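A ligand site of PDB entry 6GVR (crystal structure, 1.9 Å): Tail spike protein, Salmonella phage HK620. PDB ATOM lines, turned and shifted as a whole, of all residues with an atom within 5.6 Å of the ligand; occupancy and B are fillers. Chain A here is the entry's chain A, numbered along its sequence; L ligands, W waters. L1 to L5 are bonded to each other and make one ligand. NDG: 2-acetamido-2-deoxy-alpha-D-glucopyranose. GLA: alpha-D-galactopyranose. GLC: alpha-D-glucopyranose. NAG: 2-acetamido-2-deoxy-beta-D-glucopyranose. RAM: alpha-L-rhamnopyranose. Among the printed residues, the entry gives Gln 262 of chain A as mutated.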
ATOM      1  N   GLY A 101      14.091  -5.464   9.562  1.00  0.00           N
ATOM      2  CA  GLY A 101      13.901  -5.535   8.112  1.00  0.00           C
ATOM      3  C   GLY A 101      12.835  -6.532   7.660  1.00  0.00           C
ATOM      4  O   GLY A 101      12.436  -6.523   6.488  1.00  0.00           O
ATOM      5  N   HIS A 102      12.374  -7.411   8.567  1.00  0.00           N
ATOM      6  CA  HIS A 102      11.306  -8.320   8.314  1.00  0.00           C
ATOM      7  C   HIS A 102      10.032  -7.894   9.019  1.00  0.00           C
ATOM      8  O   HIS A 102       9.103  -8.740   9.186  1.00  0.00           O
ATOM      9  CB  HIS A 102      11.685  -9.720   8.818  1.00  0.00           C
ATOM     10  CG  HIS A 102      12.962 -10.228   8.298  1.00  0.00           C
ATOM     11  ND1 HIS A 102      13.060 -11.024   7.184  1.00  0.00           N
ATOM     12  CD2 HIS A 102      14.220 -10.109   8.775  1.00  0.00           C
ATOM     13  CE1 HIS A 102      14.307 -11.355   6.969  1.00  0.00           C
ATOM     14  NE2 HIS A 102      15.043 -10.805   7.931  1.00  0.00           N
ATOM     15  N   SER A 103       9.962  -6.627   9.464  1.00  0.00           N
ATOM     16  CA  SER A 103       8.849  -6.106  10.316  1.00  0.00           C
ATOM     17  C   SER A 103       8.614  -7.003  11.528  1.00  0.00           C
ATOM     18  O   SER A 103       7.449  -7.170  11.947  1.00  0.00           O
ATOM     19  CB  SER A 103       7.550  -6.013   9.481  1.00  0.00           C
ATOM     20  OG  SER A 103       7.781  -5.129   8.413  1.00  0.00           O
ATOM     21  N   GLN A 132       5.507  -9.480  11.368  1.00  0.00           N
ATOM     22  CA  GLN A 132       5.848 -10.908  11.394  1.00  0.00           C
ATOM     23  C   GLN A 132       6.125 -11.225  12.847  1.00  0.00           C
ATOM     24  O   GLN A 132       7.031 -10.678  13.440  1.00  0.00           O
ATOM     25  CB  GLN A 132       7.029 -11.208  10.466  1.00  0.00           C
ATOM     26  CG  GLN A 132       6.680 -11.041   8.978  1.00  0.00           C
ATOM     27  CD  GLN A 132       7.732 -11.681   8.085  1.00  0.00           C
ATOM     28  OE1 GLN A 132       7.926 -12.918   8.091  1.00  0.00           O
ATOM     29  NE2 GLN A 132       8.395 -10.861   7.246  1.00  0.00           N
ATOM     30  N   PHE A 137      15.102 -15.224  11.466  1.00  0.00           N
ATOM     31  CA  PHE A 137      16.284 -14.613  10.839  1.00  0.00           C
ATOM     32  C   PHE A 137      16.967 -13.761  11.873  1.00  0.00           C
ATOM     33  O   PHE A 137      16.325 -13.262  12.821  1.00  0.00           O
ATOM     34  CB  PHE A 137      15.969 -13.784   9.608  1.00  0.00           C
ATOM     35  CG  PHE A 137      15.273 -14.542   8.466  1.00  0.00           C
ATOM     36  CD1 PHE A 137      15.969 -15.380   7.612  1.00  0.00           C
ATOM     37  CD2 PHE A 137      13.922 -14.370   8.261  1.00  0.00           C
ATOM     38  CE1 PHE A 137      15.294 -15.994   6.546  1.00  0.00           C
ATOM     39  CE2 PHE A 137      13.245 -14.963   7.220  1.00  0.00           C
ATOM     40  CZ  PHE A 137      13.931 -15.741   6.353  1.00  0.00           C
ATOM     41  N   PRO A 142      18.231 -12.030   4.376  1.00  0.00           N
ATOM     42  CA  PRO A 142      18.284 -13.483   4.649  1.00  0.00           C
ATOM     43  C   PRO A 142      19.515 -14.230   4.139  1.00  0.00           C
ATOM     44  O   PRO A 142      20.009 -15.208   4.768  1.00  0.00           O
ATOM     45  CB  PRO A 142      16.972 -14.020   4.050  1.00  0.00           C
ATOM     46  CG  PRO A 142      16.199 -12.852   3.532  1.00  0.00           C
ATOM     47  CD  PRO A 142      16.953 -11.583   3.795  1.00  0.00           C
ATOM     48  N   LEU A 172       3.251  -7.196   3.922  1.00  0.00           N
ATOM     49  CA  LEU A 172       3.299  -8.626   4.322  1.00  0.00           C
ATOM     50  C   LEU A 172       3.003  -8.772   5.803  1.00  0.00           C
ATOM     51  O   LEU A 172       3.363  -7.915   6.636  1.00  0.00           O
ATOM     52  CB  LEU A 172       4.642  -9.236   4.035  1.00  0.00           C
ATOM     53  CG  LEU A 172       5.089  -9.152   2.594  1.00  0.00           C
ATOM     54  CD1 LEU A 172       6.584  -9.476   2.564  1.00  0.00           C
ATOM     55  CD2 LEU A 172       4.261 -10.009   1.641  1.00  0.00           C
ATOM     56  N   ASN A 174       2.919 -12.140   8.762  1.00  0.00           N
ATOM     57  CA  ASN A 174       3.251 -13.563   9.097  1.00  0.00           C
ATOM     58  C   ASN A 174       3.022 -13.779  10.611  1.00  0.00           C
ATOM     59  O   ASN A 174       3.173 -12.882  11.432  1.00  0.00           O
ATOM     60  CB  ASN A 174       4.722 -13.878   8.669  1.00  0.00           C
ATOM     61  CG  ASN A 174       5.015 -15.388   8.541  1.00  0.00           C
ATOM     62  OD1 ASN A 174       4.133 -16.249   8.770  1.00  0.00           O
ATOM     63  ND2 ASN A 174       6.263 -15.736   8.140  1.00  0.00           N
ATOM     64  N   THR A 197      -0.575 -12.731   5.289  1.00  0.00           N
ATOM     65  CA  THR A 197      -0.088 -13.298   4.055  1.00  0.00           C
ATOM     66  C   THR A 197       0.134 -14.823   4.321  1.00  0.00           C
ATOM     67  O   THR A 197      -0.246 -15.667   3.522  1.00  0.00           O
ATOM     68  CB  THR A 197       1.224 -12.691   3.676  1.00  0.00           C
ATOM     69  OG1 THR A 197       1.106 -11.248   3.587  1.00  0.00           O
ATOM     70  CG2 THR A 197       1.718 -13.249   2.389  1.00  0.00           C
ATOM     71  N   TRP A 198       0.739 -15.089   5.434  1.00  0.00           N
ATOM     72  CA  TRP A 198       0.988 -16.457   5.951  1.00  0.00           C
ATOM     73  C   TRP A 198       0.788 -16.522   7.456  1.00  0.00           C
ATOM     74  O   TRP A 198       0.862 -15.490   8.148  1.00  0.00           O
ATOM     75  CB  TRP A 198       2.407 -16.891   5.708  1.00  0.00           C
ATOM     76  CG  TRP A 198       3.011 -16.606   4.333  1.00  0.00           C
ATOM     77  CD1 TRP A 198       2.776 -17.252   3.172  1.00  0.00           C
ATOM     78  CD2 TRP A 198       3.918 -15.529   4.021  1.00  0.00           C
ATOM     79  NE1 TRP A 198       3.517 -16.702   2.159  1.00  0.00           N
ATOM     80  CE2 TRP A 198       4.241 -15.630   2.670  1.00  0.00           C
ATOM     81  CE3 TRP A 198       4.540 -14.533   4.792  1.00  0.00           C
ATOM     82  CZ2 TRP A 198       5.102 -14.756   2.053  1.00  0.00           C
ATOM     83  CZ3 TRP A 198       5.364 -13.601   4.137  1.00  0.00           C
ATOM     84  CH2 TRP A 198       5.668 -13.760   2.806  1.00  0.00           C
ATOM     85  N   THR A 201       5.913 -19.766   8.027  1.00  0.00           N
ATOM     86  CA  THR A 201       6.782 -20.107   6.915  1.00  0.00           C
ATOM     87  C   THR A 201       7.967 -20.873   7.431  1.00  0.00           C
ATOM     88  O   THR A 201       8.460 -20.554   8.516  1.00  0.00           O
ATOM     89  CB  THR A 201       7.311 -18.876   6.202  1.00  0.00           C
ATOM     90  OG1 THR A 201       8.130 -18.083   7.063  1.00  0.00           O
ATOM     91  CG2 THR A 201       6.181 -18.034   5.680  1.00  0.00           C
ATOM     92  N   LEU A 202       8.434 -21.842   6.650  1.00  0.00           N
ATOM     93  CA  LEU A 202       9.471 -22.773   7.081  1.00  0.00           C
ATOM     94  C   LEU A 202      10.600 -22.658   6.081  1.00  0.00           C
ATOM     95  O   LEU A 202      10.390 -22.672   4.885  1.00  0.00           O
ATOM     96  CB  LEU A 202       8.994 -24.194   7.112  1.00  0.00           C
ATOM     97  CG  LEU A 202       7.724 -24.524   7.842  1.00  0.00           C
ATOM     98  CD1 LEU A 202       7.506 -26.060   7.710  1.00  0.00           C
ATOM     99  CD2 LEU A 202       7.709 -24.054   9.274  1.00  0.00           C
ATOM    100  N   GLY A 203      11.800 -22.498   6.557  1.00  0.00           N
ATOM    101  CA  GLY A 203      12.910 -22.406   5.607  1.00  0.00           C
ATOM    102  C   GLY A 203      12.999 -21.045   4.889  1.00  0.00           C
ATOM    103  O   GLY A 203      12.104 -20.135   5.063  1.00  0.00           O
ATOM    104  N   TRP A 204      14.055 -20.921   4.113  1.00  0.00           N
ATOM    105  CA  TRP A 204      14.272 -19.731   3.217  1.00  0.00           C
ATOM    106  C   TRP A 204      15.001 -20.220   2.010  1.00  0.00           C
ATOM    107  O   TRP A 204      16.177 -20.654   2.137  1.00  0.00           O
ATOM    108  CB  TRP A 204      15.017 -18.591   3.906  1.00  0.00           C
ATOM    109  CG  TRP A 204      15.302 -17.494   2.941  1.00  0.00           C
ATOM    110  CD1 TRP A 204      14.395 -16.651   2.396  1.00  0.00           C
ATOM    111  CD2 TRP A 204      16.566 -17.211   2.280  1.00  0.00           C
ATOM    112  NE1 TRP A 204      15.007 -15.792   1.475  1.00  0.00           N
ATOM    113  CE2 TRP A 204      16.331 -16.141   1.359  1.00  0.00           C
ATOM    114  CE3 TRP A 204      17.844 -17.729   2.380  1.00  0.00           C
ATOM    115  CZ2 TRP A 204      17.318 -15.613   0.567  1.00  0.00           C
ATOM    116  CZ3 TRP A 204      18.841 -17.219   1.594  1.00  0.00           C
ATOM    117  CH2 TRP A 204      18.572 -16.129   0.697  1.00  0.00           C
ATOM    118  N   ASN A 205      14.330 -20.150   0.858  1.00  0.00           N
ATOM    119  CA  ASN A 205      14.900 -20.529  -0.430  1.00  0.00           C
ATOM    120  C   ASN A 205      15.753 -21.778  -0.402  1.00  0.00           C
ATOM    121  O   ASN A 205      16.878 -21.849  -0.905  1.00  0.00           O
ATOM    122  CB  ASN A 205      15.622 -19.348  -1.030  1.00  0.00           C
ATOM    123  CG  ASN A 205      14.691 -18.208  -1.396  1.00  0.00           C
ATOM    124  OD1 ASN A 205      13.443 -18.241  -1.162  1.00  0.00           O
ATOM    125  ND2 ASN A 205      15.313 -17.101  -1.806  1.00  0.00           N
ATOM    126  N   ASP A 229      -2.992 -11.761  -1.176  1.00  0.00           N
ATOM    127  CA  ASP A 229      -2.682 -13.185  -1.382  1.00  0.00           C
ATOM    128  C   ASP A 229      -2.420 -13.829  -0.049  1.00  0.00           C
ATOM    129  O   ASP A 229      -1.837 -13.189   0.862  1.00  0.00           O
ATOM    130  CB  ASP A 229      -1.432 -13.294  -2.259  1.00  0.00           C
ATOM    131  CG  ASP A 229      -1.267 -14.649  -2.864  1.00  0.00           C
ATOM    132  OD1 ASP A 229      -2.107 -15.630  -2.639  1.00  0.00           O
ATOM    133  OD2 ASP A 229      -0.254 -14.700  -3.559  1.00  0.00           O
ATOM    134  N   HIS A 230      -2.820 -15.072   0.105  1.00  0.00           N
ATOM    135  CA  HIS A 230      -2.596 -15.760   1.345  1.00  0.00           C
ATOM    136  C   HIS A 230      -2.269 -17.242   1.103  1.00  0.00           C
ATOM    137  O   HIS A 230      -2.912 -17.903   0.323  1.00  0.00           O
ATOM    138  CB  HIS A 230      -3.802 -15.678   2.278  1.00  0.00           C
ATOM    139  CG  HIS A 230      -3.678 -16.533   3.499  1.00  0.00           C
ATOM    140  ND1 HIS A 230      -3.355 -16.017   4.750  1.00  0.00           N
ATOM    141  CD2 HIS A 230      -3.893 -17.858   3.669  1.00  0.00           C
ATOM    142  CE1 HIS A 230      -3.350 -17.026   5.610  1.00  0.00           C
ATOM    143  NE2 HIS A 230      -3.674 -18.144   4.977  1.00  0.00           N
ATOM    144  N   SER A 231      -1.238 -17.700   1.810  1.00  0.00           N
ATOM    145  CA  SER A 231      -0.909 -19.164   1.879  1.00  0.00           C
ATOM    146  C   SER A 231      -0.619 -19.446   3.335  1.00  0.00           C
ATOM    147  O   SER A 231       0.312 -18.828   3.887  1.00  0.00           O
ATOM    148  CB  SER A 231       0.293 -19.516   1.003  1.00  0.00           C
ATOM    149  OG  SER A 231      -0.073 -19.392  -0.381  1.00  0.00           O
ATOM    150  N   TYR A 234       3.914 -21.992   4.335  1.00  0.00           N
ATOM    151  CA  TYR A 234       4.802 -21.996   3.167  1.00  0.00           C
ATOM    152  C   TYR A 234       6.027 -22.823   3.539  1.00  0.00           C
ATOM    153  O   TYR A 234       6.799 -22.477   4.458  1.00  0.00           O
ATOM    154  CB  TYR A 234       5.255 -20.576   2.813  1.00  0.00           C
ATOM    155  CG  TYR A 234       5.755 -20.300   1.405  1.00  0.00           C
ATOM    156  CD1 TYR A 234       6.984 -20.784   0.969  1.00  0.00           C
ATOM    157  CD2 TYR A 234       5.027 -19.510   0.500  1.00  0.00           C
ATOM    158  CE1 TYR A 234       7.446 -20.500  -0.317  1.00  0.00           C
ATOM    159  CE2 TYR A 234       5.494 -19.218  -0.768  1.00  0.00           C
ATOM    160  CZ  TYR A 234       6.747 -19.660  -1.163  1.00  0.00           C
ATOM    161  OH  TYR A 234       7.224 -19.324  -2.408  1.00  0.00           O
ATOM    162  N   ASN A 236       9.466 -24.012   2.630  1.00  0.00           N
ATOM    163  CA  ASN A 236      10.583 -23.590   1.733  1.00  0.00           C
ATOM    164  C   ASN A 236      11.941 -24.137   2.176  1.00  0.00           C
ATOM    165  O   ASN A 236      13.032 -23.636   1.855  1.00  0.00           O
ATOM    166  CB  ASN A 236      10.607 -22.085   1.618  1.00  0.00           C
ATOM    167  CG  ASN A 236      11.180 -21.579   0.300  1.00  0.00           C
ATOM    168  OD1 ASN A 236      11.470 -22.342  -0.614  1.00  0.00           O
ATOM    169  ND2 ASN A 236      11.402 -20.203   0.219  1.00  0.00           N
ATOM    170  N   GLN A 262       1.937 -24.336   0.794  1.00  0.00           N
ATOM    171  CA  GLN A 262       2.883 -24.265  -0.335  1.00  0.00           C
ATOM    172  C   GLN A 262       3.962 -25.332  -0.094  1.00  0.00           C
ATOM    173  O   GLN A 262       4.649 -25.193   0.912  1.00  0.00           O
ATOM    174  CB  GLN A 262       3.572 -22.850  -0.428  1.00  0.00           C
ATOM    175  CG  GLN A 262       2.563 -21.699  -0.660  1.00  0.00           C
ATOM    176  CD  GLN A 262       1.986 -21.565  -2.098  1.00  0.00           C
ATOM    177  OE1 GLN A 262       0.827 -21.086  -2.251  1.00  0.00           O
ATOM    178  NE2 GLN A 262       2.761 -21.900  -3.138  1.00  0.00           N
ATOM    179  N   HIS A 264       7.429 -26.291  -1.573  1.00  0.00           N
ATOM    180  CA  HIS A 264       8.310 -25.663  -2.550  1.00  0.00           C
ATOM    181  C   HIS A 264       9.706 -26.197  -2.546  1.00  0.00           C
ATOM    182  O   HIS A 264      10.563 -25.580  -3.226  1.00  0.00           O
ATOM    183  CB  HIS A 264       8.367 -24.170  -2.350  1.00  0.00           C
ATOM    184  CG  HIS A 264       7.224 -23.443  -2.929  1.00  0.00           C
ATOM    185  ND1 HIS A 264       7.368 -22.228  -3.564  1.00  0.00           N
ATOM    186  CD2 HIS A 264       5.916 -23.761  -3.037  1.00  0.00           C
ATOM    187  CE1 HIS A 264       6.189 -21.811  -4.002  1.00  0.00           C
ATOM    188  NE2 HIS A 264       5.281 -22.679  -3.637  1.00  0.00           N
ATOM    189  N   TYR A 283      -0.177 -25.651  -3.450  1.00  0.00           N
ATOM    190  CA  TYR A 283       0.703 -25.539  -4.601  1.00  0.00           C
ATOM    191  C   TYR A 283       1.913 -26.464  -4.374  1.00  0.00           C
ATOM    192  O   TYR A 283       2.438 -26.516  -3.265  1.00  0.00           O
ATOM    193  CB  TYR A 283       1.224 -24.135  -4.775  1.00  0.00           C
ATOM    194  CG  TYR A 283       0.234 -23.123  -5.325  1.00  0.00           C
ATOM    195  CD1 TYR A 283      -0.675 -22.484  -4.476  1.00  0.00           C
ATOM    196  CD2 TYR A 283       0.252 -22.756  -6.697  1.00  0.00           C
ATOM    197  CE1 TYR A 283      -1.532 -21.450  -4.963  1.00  0.00           C
ATOM    198  CE2 TYR A 283      -0.671 -21.779  -7.184  1.00  0.00           C
ATOM    199  CZ  TYR A 283      -1.554 -21.152  -6.314  1.00  0.00           C
ATOM    200  OH  TYR A 283      -2.417 -20.175  -6.807  1.00  0.00           O
ATOM    201  N   VAL A 285       5.367 -26.792  -6.183  1.00  0.00           N
ATOM    202  CA  VAL A 285       6.004 -25.888  -7.178  1.00  0.00           C
ATOM    203  C   VAL A 285       7.496 -25.849  -6.930  1.00  0.00           C
ATOM    204  O   VAL A 285       7.877 -25.654  -5.766  1.00  0.00           O
ATOM    205  CB  VAL A 285       5.463 -24.421  -7.070  1.00  0.00           C
ATOM    206  CG1 VAL A 285       6.312 -23.440  -7.914  1.00  0.00           C
ATOM    207  CG2 VAL A 285       4.035 -24.316  -7.541  1.00  0.00           C
ATOM    208  N   HIS A 287      10.195 -23.167  -7.721  1.00  0.00           N
ATOM    209  CA  HIS A 287      10.516 -21.830  -8.271  1.00  0.00           C
ATOM    210  C   HIS A 287      12.063 -21.764  -8.440  1.00  0.00           C
ATOM    211  O   HIS A 287      12.799 -21.834  -7.467  1.00  0.00           O
ATOM    212  CB  HIS A 287      10.114 -20.709  -7.328  1.00  0.00           C
ATOM    213  CG  HIS A 287       8.654 -20.338  -7.295  1.00  0.00           C
ATOM    214  ND1 HIS A 287       7.907 -20.119  -8.424  1.00  0.00           N
ATOM    215  CD2 HIS A 287       7.886 -19.913  -6.253  1.00  0.00           C
ATOM    216  CE1 HIS A 287       6.690 -19.718  -8.078  1.00  0.00           C
ATOM    217  NE2 HIS A 287       6.638 -19.618  -6.762  1.00  0.00           N
ATOM    218  N   ALA A 289      13.775 -19.235  -8.577  1.00  0.00           N
ATOM    219  CA  ALA A 289      14.202 -18.224  -7.652  1.00  0.00           C
ATOM    220  C   ALA A 289      14.416 -18.648  -6.211  1.00  0.00           C
ATOM    221  O   ALA A 289      15.034 -17.908  -5.425  1.00  0.00           O
ATOM    222  CB  ALA A 289      13.261 -17.020  -7.724  1.00  0.00           C
ATOM    223  N   GLU A 290      13.967 -19.835  -5.827  1.00  0.00           N
ATOM    224  CA  GLU A 290      14.067 -20.301  -4.492  1.00  0.00           C
ATOM    225  C   GLU A 290      14.983 -21.485  -4.399  1.00  0.00           C
ATOM    226  O   GLU A 290      14.915 -22.289  -3.440  1.00  0.00           O
ATOM    227  CB  GLU A 290      12.621 -20.734  -4.003  1.00  0.00           C
ATOM    228  CG  GLU A 290      11.652 -19.559  -3.940  1.00  0.00           C
ATOM    229  CD  GLU A 290      10.294 -19.947  -3.407  1.00  0.00           C
ATOM    230  OE1 GLU A 290       9.883 -21.113  -3.696  1.00  0.00           O
ATOM    231  OE2 GLU A 290       9.664 -19.077  -2.782  1.00  0.00           O
ATOM    232  N   PRO A 359       2.037 -22.659 -12.600  1.00  0.00           N
ATOM    233  CA  PRO A 359       1.157 -21.733 -11.799  1.00  0.00           C
ATOM    234  C   PRO A 359       0.963 -20.331 -12.541  1.00  0.00           C
ATOM    235  O   PRO A 359      -0.156 -19.929 -12.945  1.00  0.00           O
ATOM    236  CB  PRO A 359       1.973 -21.568 -10.478  1.00  0.00           C
ATOM    237  CG  PRO A 359       3.459 -21.841 -10.861  1.00  0.00           C
ATOM    238  CD  PRO A 359       3.478 -22.369 -12.302  1.00  0.00           C
HETATM  239  C1  NDG L   1       1.092 -18.520  -4.100  1.00  0.00           C
HETATM  240  C2  NDG L   1       2.222 -17.799  -3.335  1.00  0.00           C
HETATM  241  C3  NDG L   1       3.250 -17.218  -4.335  1.00  0.00           C
HETATM  242  C4  NDG L   1       3.744 -18.352  -5.243  1.00  0.00           C
HETATM  243  C5  NDG L   1       2.559 -19.049  -5.945  1.00  0.00           C
HETATM  244  C6  NDG L   1       2.902 -20.269  -6.734  1.00  0.00           C
HETATM  245  C7  NDG L   1       1.849 -16.726  -1.123  1.00  0.00           C
HETATM  246  C8  NDG L   1       1.063 -15.712  -0.380  1.00  0.00           C
HETATM  247  O5  NDG L   1       1.620 -19.505  -4.995  1.00  0.00           O
HETATM  248  O3  NDG L   1       4.386 -16.684  -3.578  1.00  0.00           O
HETATM  249  O4  NDG L   1       4.750 -17.959  -6.196  1.00  0.00           O
HETATM  250  O6  NDG L   1       3.367 -21.202  -5.729  1.00  0.00           O
HETATM  251  O7  NDG L   1       2.692 -17.426  -0.545  1.00  0.00           O
HETATM  252  N2  NDG L   1       1.627 -16.803  -2.458  1.00  0.00           N
HETATM  253  O1  NDG L   1       0.410 -17.607  -4.904  1.00  0.00           O
HETATM  254  C1  GLA L   2       5.019 -15.554  -4.185  1.00  0.00           C
HETATM  255  C2  GLA L   2       6.420 -15.521  -3.621  1.00  0.00           C
HETATM  256  C3  GLA L   2       6.446 -15.250  -2.098  1.00  0.00           C
HETATM  257  C4  GLA L   2       5.557 -14.054  -1.749  1.00  0.00           C
HETATM  258  C5  GLA L   2       4.160 -14.234  -2.372  1.00  0.00           C
HETATM  259  C6  GLA L   2       3.186 -13.085  -2.169  1.00  0.00           C
HETATM  260  O2  GLA L   2       7.077 -16.782  -3.893  1.00  0.00           O
HETATM  261  O3  GLA L   2       7.823 -15.029  -1.750  1.00  0.00           O
HETATM  262  O4  GLA L   2       6.149 -12.846  -2.299  1.00  0.00           O
HETATM  263  O5  GLA L   2       4.290 -14.462  -3.790  1.00  0.00           O
HETATM  264  O6  GLA L   2       3.104 -12.833  -0.777  1.00  0.00           O
HETATM  265  C1  GLC L   3       6.193 -11.780  -1.306  1.00  0.00           C
HETATM  266  C2  GLC L   3       6.578 -10.448  -1.998  1.00  0.00           C
HETATM  267  C3  GLC L   3       7.975 -10.482  -2.623  1.00  0.00           C
HETATM  268  C4  GLC L   3       8.896 -10.809  -1.509  1.00  0.00           C
HETATM  269  C5  GLC L   3       8.509 -12.139  -0.862  1.00  0.00           C
HETATM  270  C6  GLC L   3       9.444 -12.549   0.285  1.00  0.00           C
HETATM  271  O2  GLC L   3       5.661 -10.157  -2.972  1.00  0.00           O
HETATM  272  O3  GLC L   3       8.281  -9.174  -3.064  1.00  0.00           O
HETATM  273  O4  GLC L   3      10.209 -10.786  -1.998  1.00  0.00           O
HETATM  274  O5  GLC L   3       7.158 -12.039  -0.316  1.00  0.00           O
HETATM  275  O6  GLC L   3       9.456 -11.573   1.375  1.00  0.00           O
HETATM  276  C1  NAG L   4       8.352 -16.079  -0.939  1.00  0.00           C
HETATM  277  C2  NAG L   4       9.869 -16.022  -1.026  1.00  0.00           C
HETATM  278  C3  NAG L   4      10.537 -17.023  -0.097  1.00  0.00           C
HETATM  279  C4  NAG L   4       9.942 -17.035   1.276  1.00  0.00           C
HETATM  280  C5  NAG L   4       8.465 -17.168   1.111  1.00  0.00           C
HETATM  281  C6  NAG L   4       7.794 -17.325   2.436  1.00  0.00           C
HETATM  282  C7  NAG L   4      10.880 -15.388  -3.140  1.00  0.00           C
HETATM  283  C8  NAG L   4      11.169 -15.731  -4.588  1.00  0.00           C
HETATM  284  N2  NAG L   4      10.218 -16.282  -2.393  1.00  0.00           N
HETATM  285  O3  NAG L   4      11.866 -16.615  -0.013  1.00  0.00           O
HETATM  286  O4  NAG L   4      10.431 -18.207   1.938  1.00  0.00           O
HETATM  287  O5  NAG L   4       7.926 -16.009   0.425  1.00  0.00           O
HETATM  288  O6  NAG L   4       7.950 -16.119   3.115  1.00  0.00           O
HETATM  289  O7  NAG L   4      11.312 -14.355  -2.660  1.00  0.00           O
HETATM  290  C1  RAM L   5      10.786 -11.019   1.539  1.00  0.00           C
HETATM  291  C2  RAM L   5      10.664  -9.798   2.455  1.00  0.00           C
HETATM  292  C3  RAM L   5      10.308 -10.176   3.888  1.00  0.00           C
HETATM  293  C4  RAM L   5      11.248 -11.302   4.358  1.00  0.00           C
HETATM  294  C5  RAM L   5      11.352 -12.437   3.318  1.00  0.00           C
HETATM  295  C6  RAM L   5      12.376 -13.535   3.669  1.00  0.00           C
HETATM  296  O2  RAM L   5      11.938  -9.188   2.359  1.00  0.00           O
HETATM  297  O3  RAM L   5      10.343  -8.997   4.741  1.00  0.00           O
HETATM  298  O4  RAM L   5      10.835 -11.726   5.670  1.00  0.00           O
HETATM  299  O5  RAM L   5      11.745 -11.950   2.028  1.00  0.00           O
HETATM  300  O   HOH W   1      11.615 -17.473   4.278  1.00  0.00           O
HETATM  301  O   HOH W   2       9.523 -16.266   5.477  1.00  0.00           O
HETATM  302  O   HOH W   3       4.361  -8.103  -2.024  1.00  0.00           O
HETATM  303  O   HOH W   4      10.497  -8.720  -4.629  1.00  0.00           O
HETATM  304  O   HOH W   5      14.130  -8.725   4.620  1.00  0.00           O
HETATM  305  O   HOH W   6       1.223 -10.859  -0.688  1.00  0.00           O
HETATM  306  O   HOH W   7       4.292 -16.374  -8.152  1.00  0.00           O
HETATM  307  O   HOH W   8      13.003 -13.954   0.260  1.00  0.00           O
HETATM  308  O   HOH W   9       5.633 -12.077  -5.176  1.00  0.00           O
HETATM  309  O   HOH W  10      12.133  -8.461  -0.223  1.00  0.00           O
HETATM  310  O   HOH W  11      14.040 -14.540  -2.239  1.00  0.00           O
HETATM  311  O   HOH W  12       7.995  -7.662   5.959  1.00  0.00           O
HETATM  312  O   HOH W  13      -2.167 -17.674  -5.393  1.00  0.00           O
HETATM  313  O   HOH W  14       8.000 -16.262  -6.453  1.00  0.00           O
HETATM  314  O   HOH W  15       9.819 -13.911   6.830  1.00  0.00           O
HETATM  315  O   HOH W  16      10.702  -6.457   3.937  1.00  0.00           O
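Gly 101 touches the ligand.
CZ of Phe 137 touches C6 of RAM L5, 3.8 Å away.
CG of Pro 142 touches C6 of RAM L5 (3.9 Å).
CD1 of Leu 172 touches O6 of GLC L3 (3.7 Å).
CG2 of Thr 197 touches O6 of GLA L2, 3.5 Å away.
Thr 201 touches the ligand.
CD1 of Trp 204 touches O3 of NAG L4, 3.5 Å away.
C of His 230 touches C8 of NDG L1, 3.96 Å away.
CD2 of Tyr 283 touches O6 of NDG L1 (3.6 Å).
CG2 of Val 285 touches O6 of NDG L1, 3.7 Å away.
CB of Ala 289 touches C8 of NAG L4, 3.98 Å away.
Water W13 lies within hydrogen-bond range of O1 of NDG L1, OH of Tyr 283 and OD1 of Asp 229.
Water W15 lies within hydrogen-bond range of OE1 of Gln 132 and O4 of RAM L5.
Water W1 bridges O4 of NAG L4 (2.7 Å) and O of Gly 203 (2.8 Å).
Water W11 bridges O7 of NAG L4 (2.8 Å) and ND2 of Asn 205 (2.9 Å).
Water W8 bridges O3 of NAG L4 (2.9 Å) and NE1 of Trp 204 (3.0 Å).
Water W12 bridges an oxygen (O3) of RAM L5 and the side-chain amide nitrogen (NE2) of Gln 132.
The side-chain amide nitrogen (NE2) of Gln 262 sits at hydrogen-bond distance from a ring nitrogen (NE2) of His 264, at 2.7 Å.
The side-chain amide oxygen (OE1) of Gln 262 is in hydrogen-bond range of the side-chain hydroxyl (OG) of Ser 231, at 2.7 Å.
O of His 102 lies within hydrogen-bond range of NE2 of Gln 132, 3.0 Å away.
ND1 of His 264 sits at hydrogen-bond distance from OE1 of Glu 290 (2.8 Å).
OD1 of Asn 174 lies close to O of Trp 198 (3.4 Å).
ND1 of His 264 is in hydrogen-bond range of OH of Tyr 234 (3.1 Å).
The backbone NH (N) of Gln 132 sits at hydrogen-bond distance from the backbone carbonyl oxygen (O) of Ser 103, at 3.1 Å.
OG1 of Thr 201 is in hydrogen-bond range of ND2 of Asn 174 (3.2 Å).
OD1 of Asn 205 sits at hydrogen-bond distance from O3 of NAG L4 (2.5 Å).
A ring nitrogen (NE2) of His 287 sits at hydrogen-bond distance from an oxygen (O4) of NDG L1.
An oxygen (O6) of NDG L1 lies within hydrogen-bond range of the side-chain amide nitrogen of Gln 262 (2.8 Å).
O4 of RAM L5 sits at hydrogen-bond distance from ND1 of His 102 (2.8 Å).
The side-chain amide nitrogen (ND2) of Asn 236 sits at hydrogen-bond distance from an oxygen (O4) of NAG L4.
The side-chain carboxylate (OE2) of Glu 290 lies within hydrogen-bond range of a nitrogen (N2) of NAG L4 (2.9 Å).
The indole nitrogen (NE1) of Trp 198 lies within hydrogen-bond range of an oxygen (O7) of NDG L1 (2.9 Å).
The side-chain hydroxyl (OH) of Tyr 234 is in hydrogen-bond range of an oxygen (O2) of GLA L2 (2.9 Å).
OD2 of Asp 229 is in hydrogen-bond range of N2 of NDG L1, 3.0 Å away.
O4 of RAM L5 sits at hydrogen-bond distance from NE2 of Gln 132 (3.0 Å).
O6 of NDG L1 sits at hydrogen-bond distance from NE2 of His 264, at 3.2 Å.
An oxygen (O7) of NDG L1 lies close to the side-chain hydroxyl of Ser 231 (3.4 Å).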
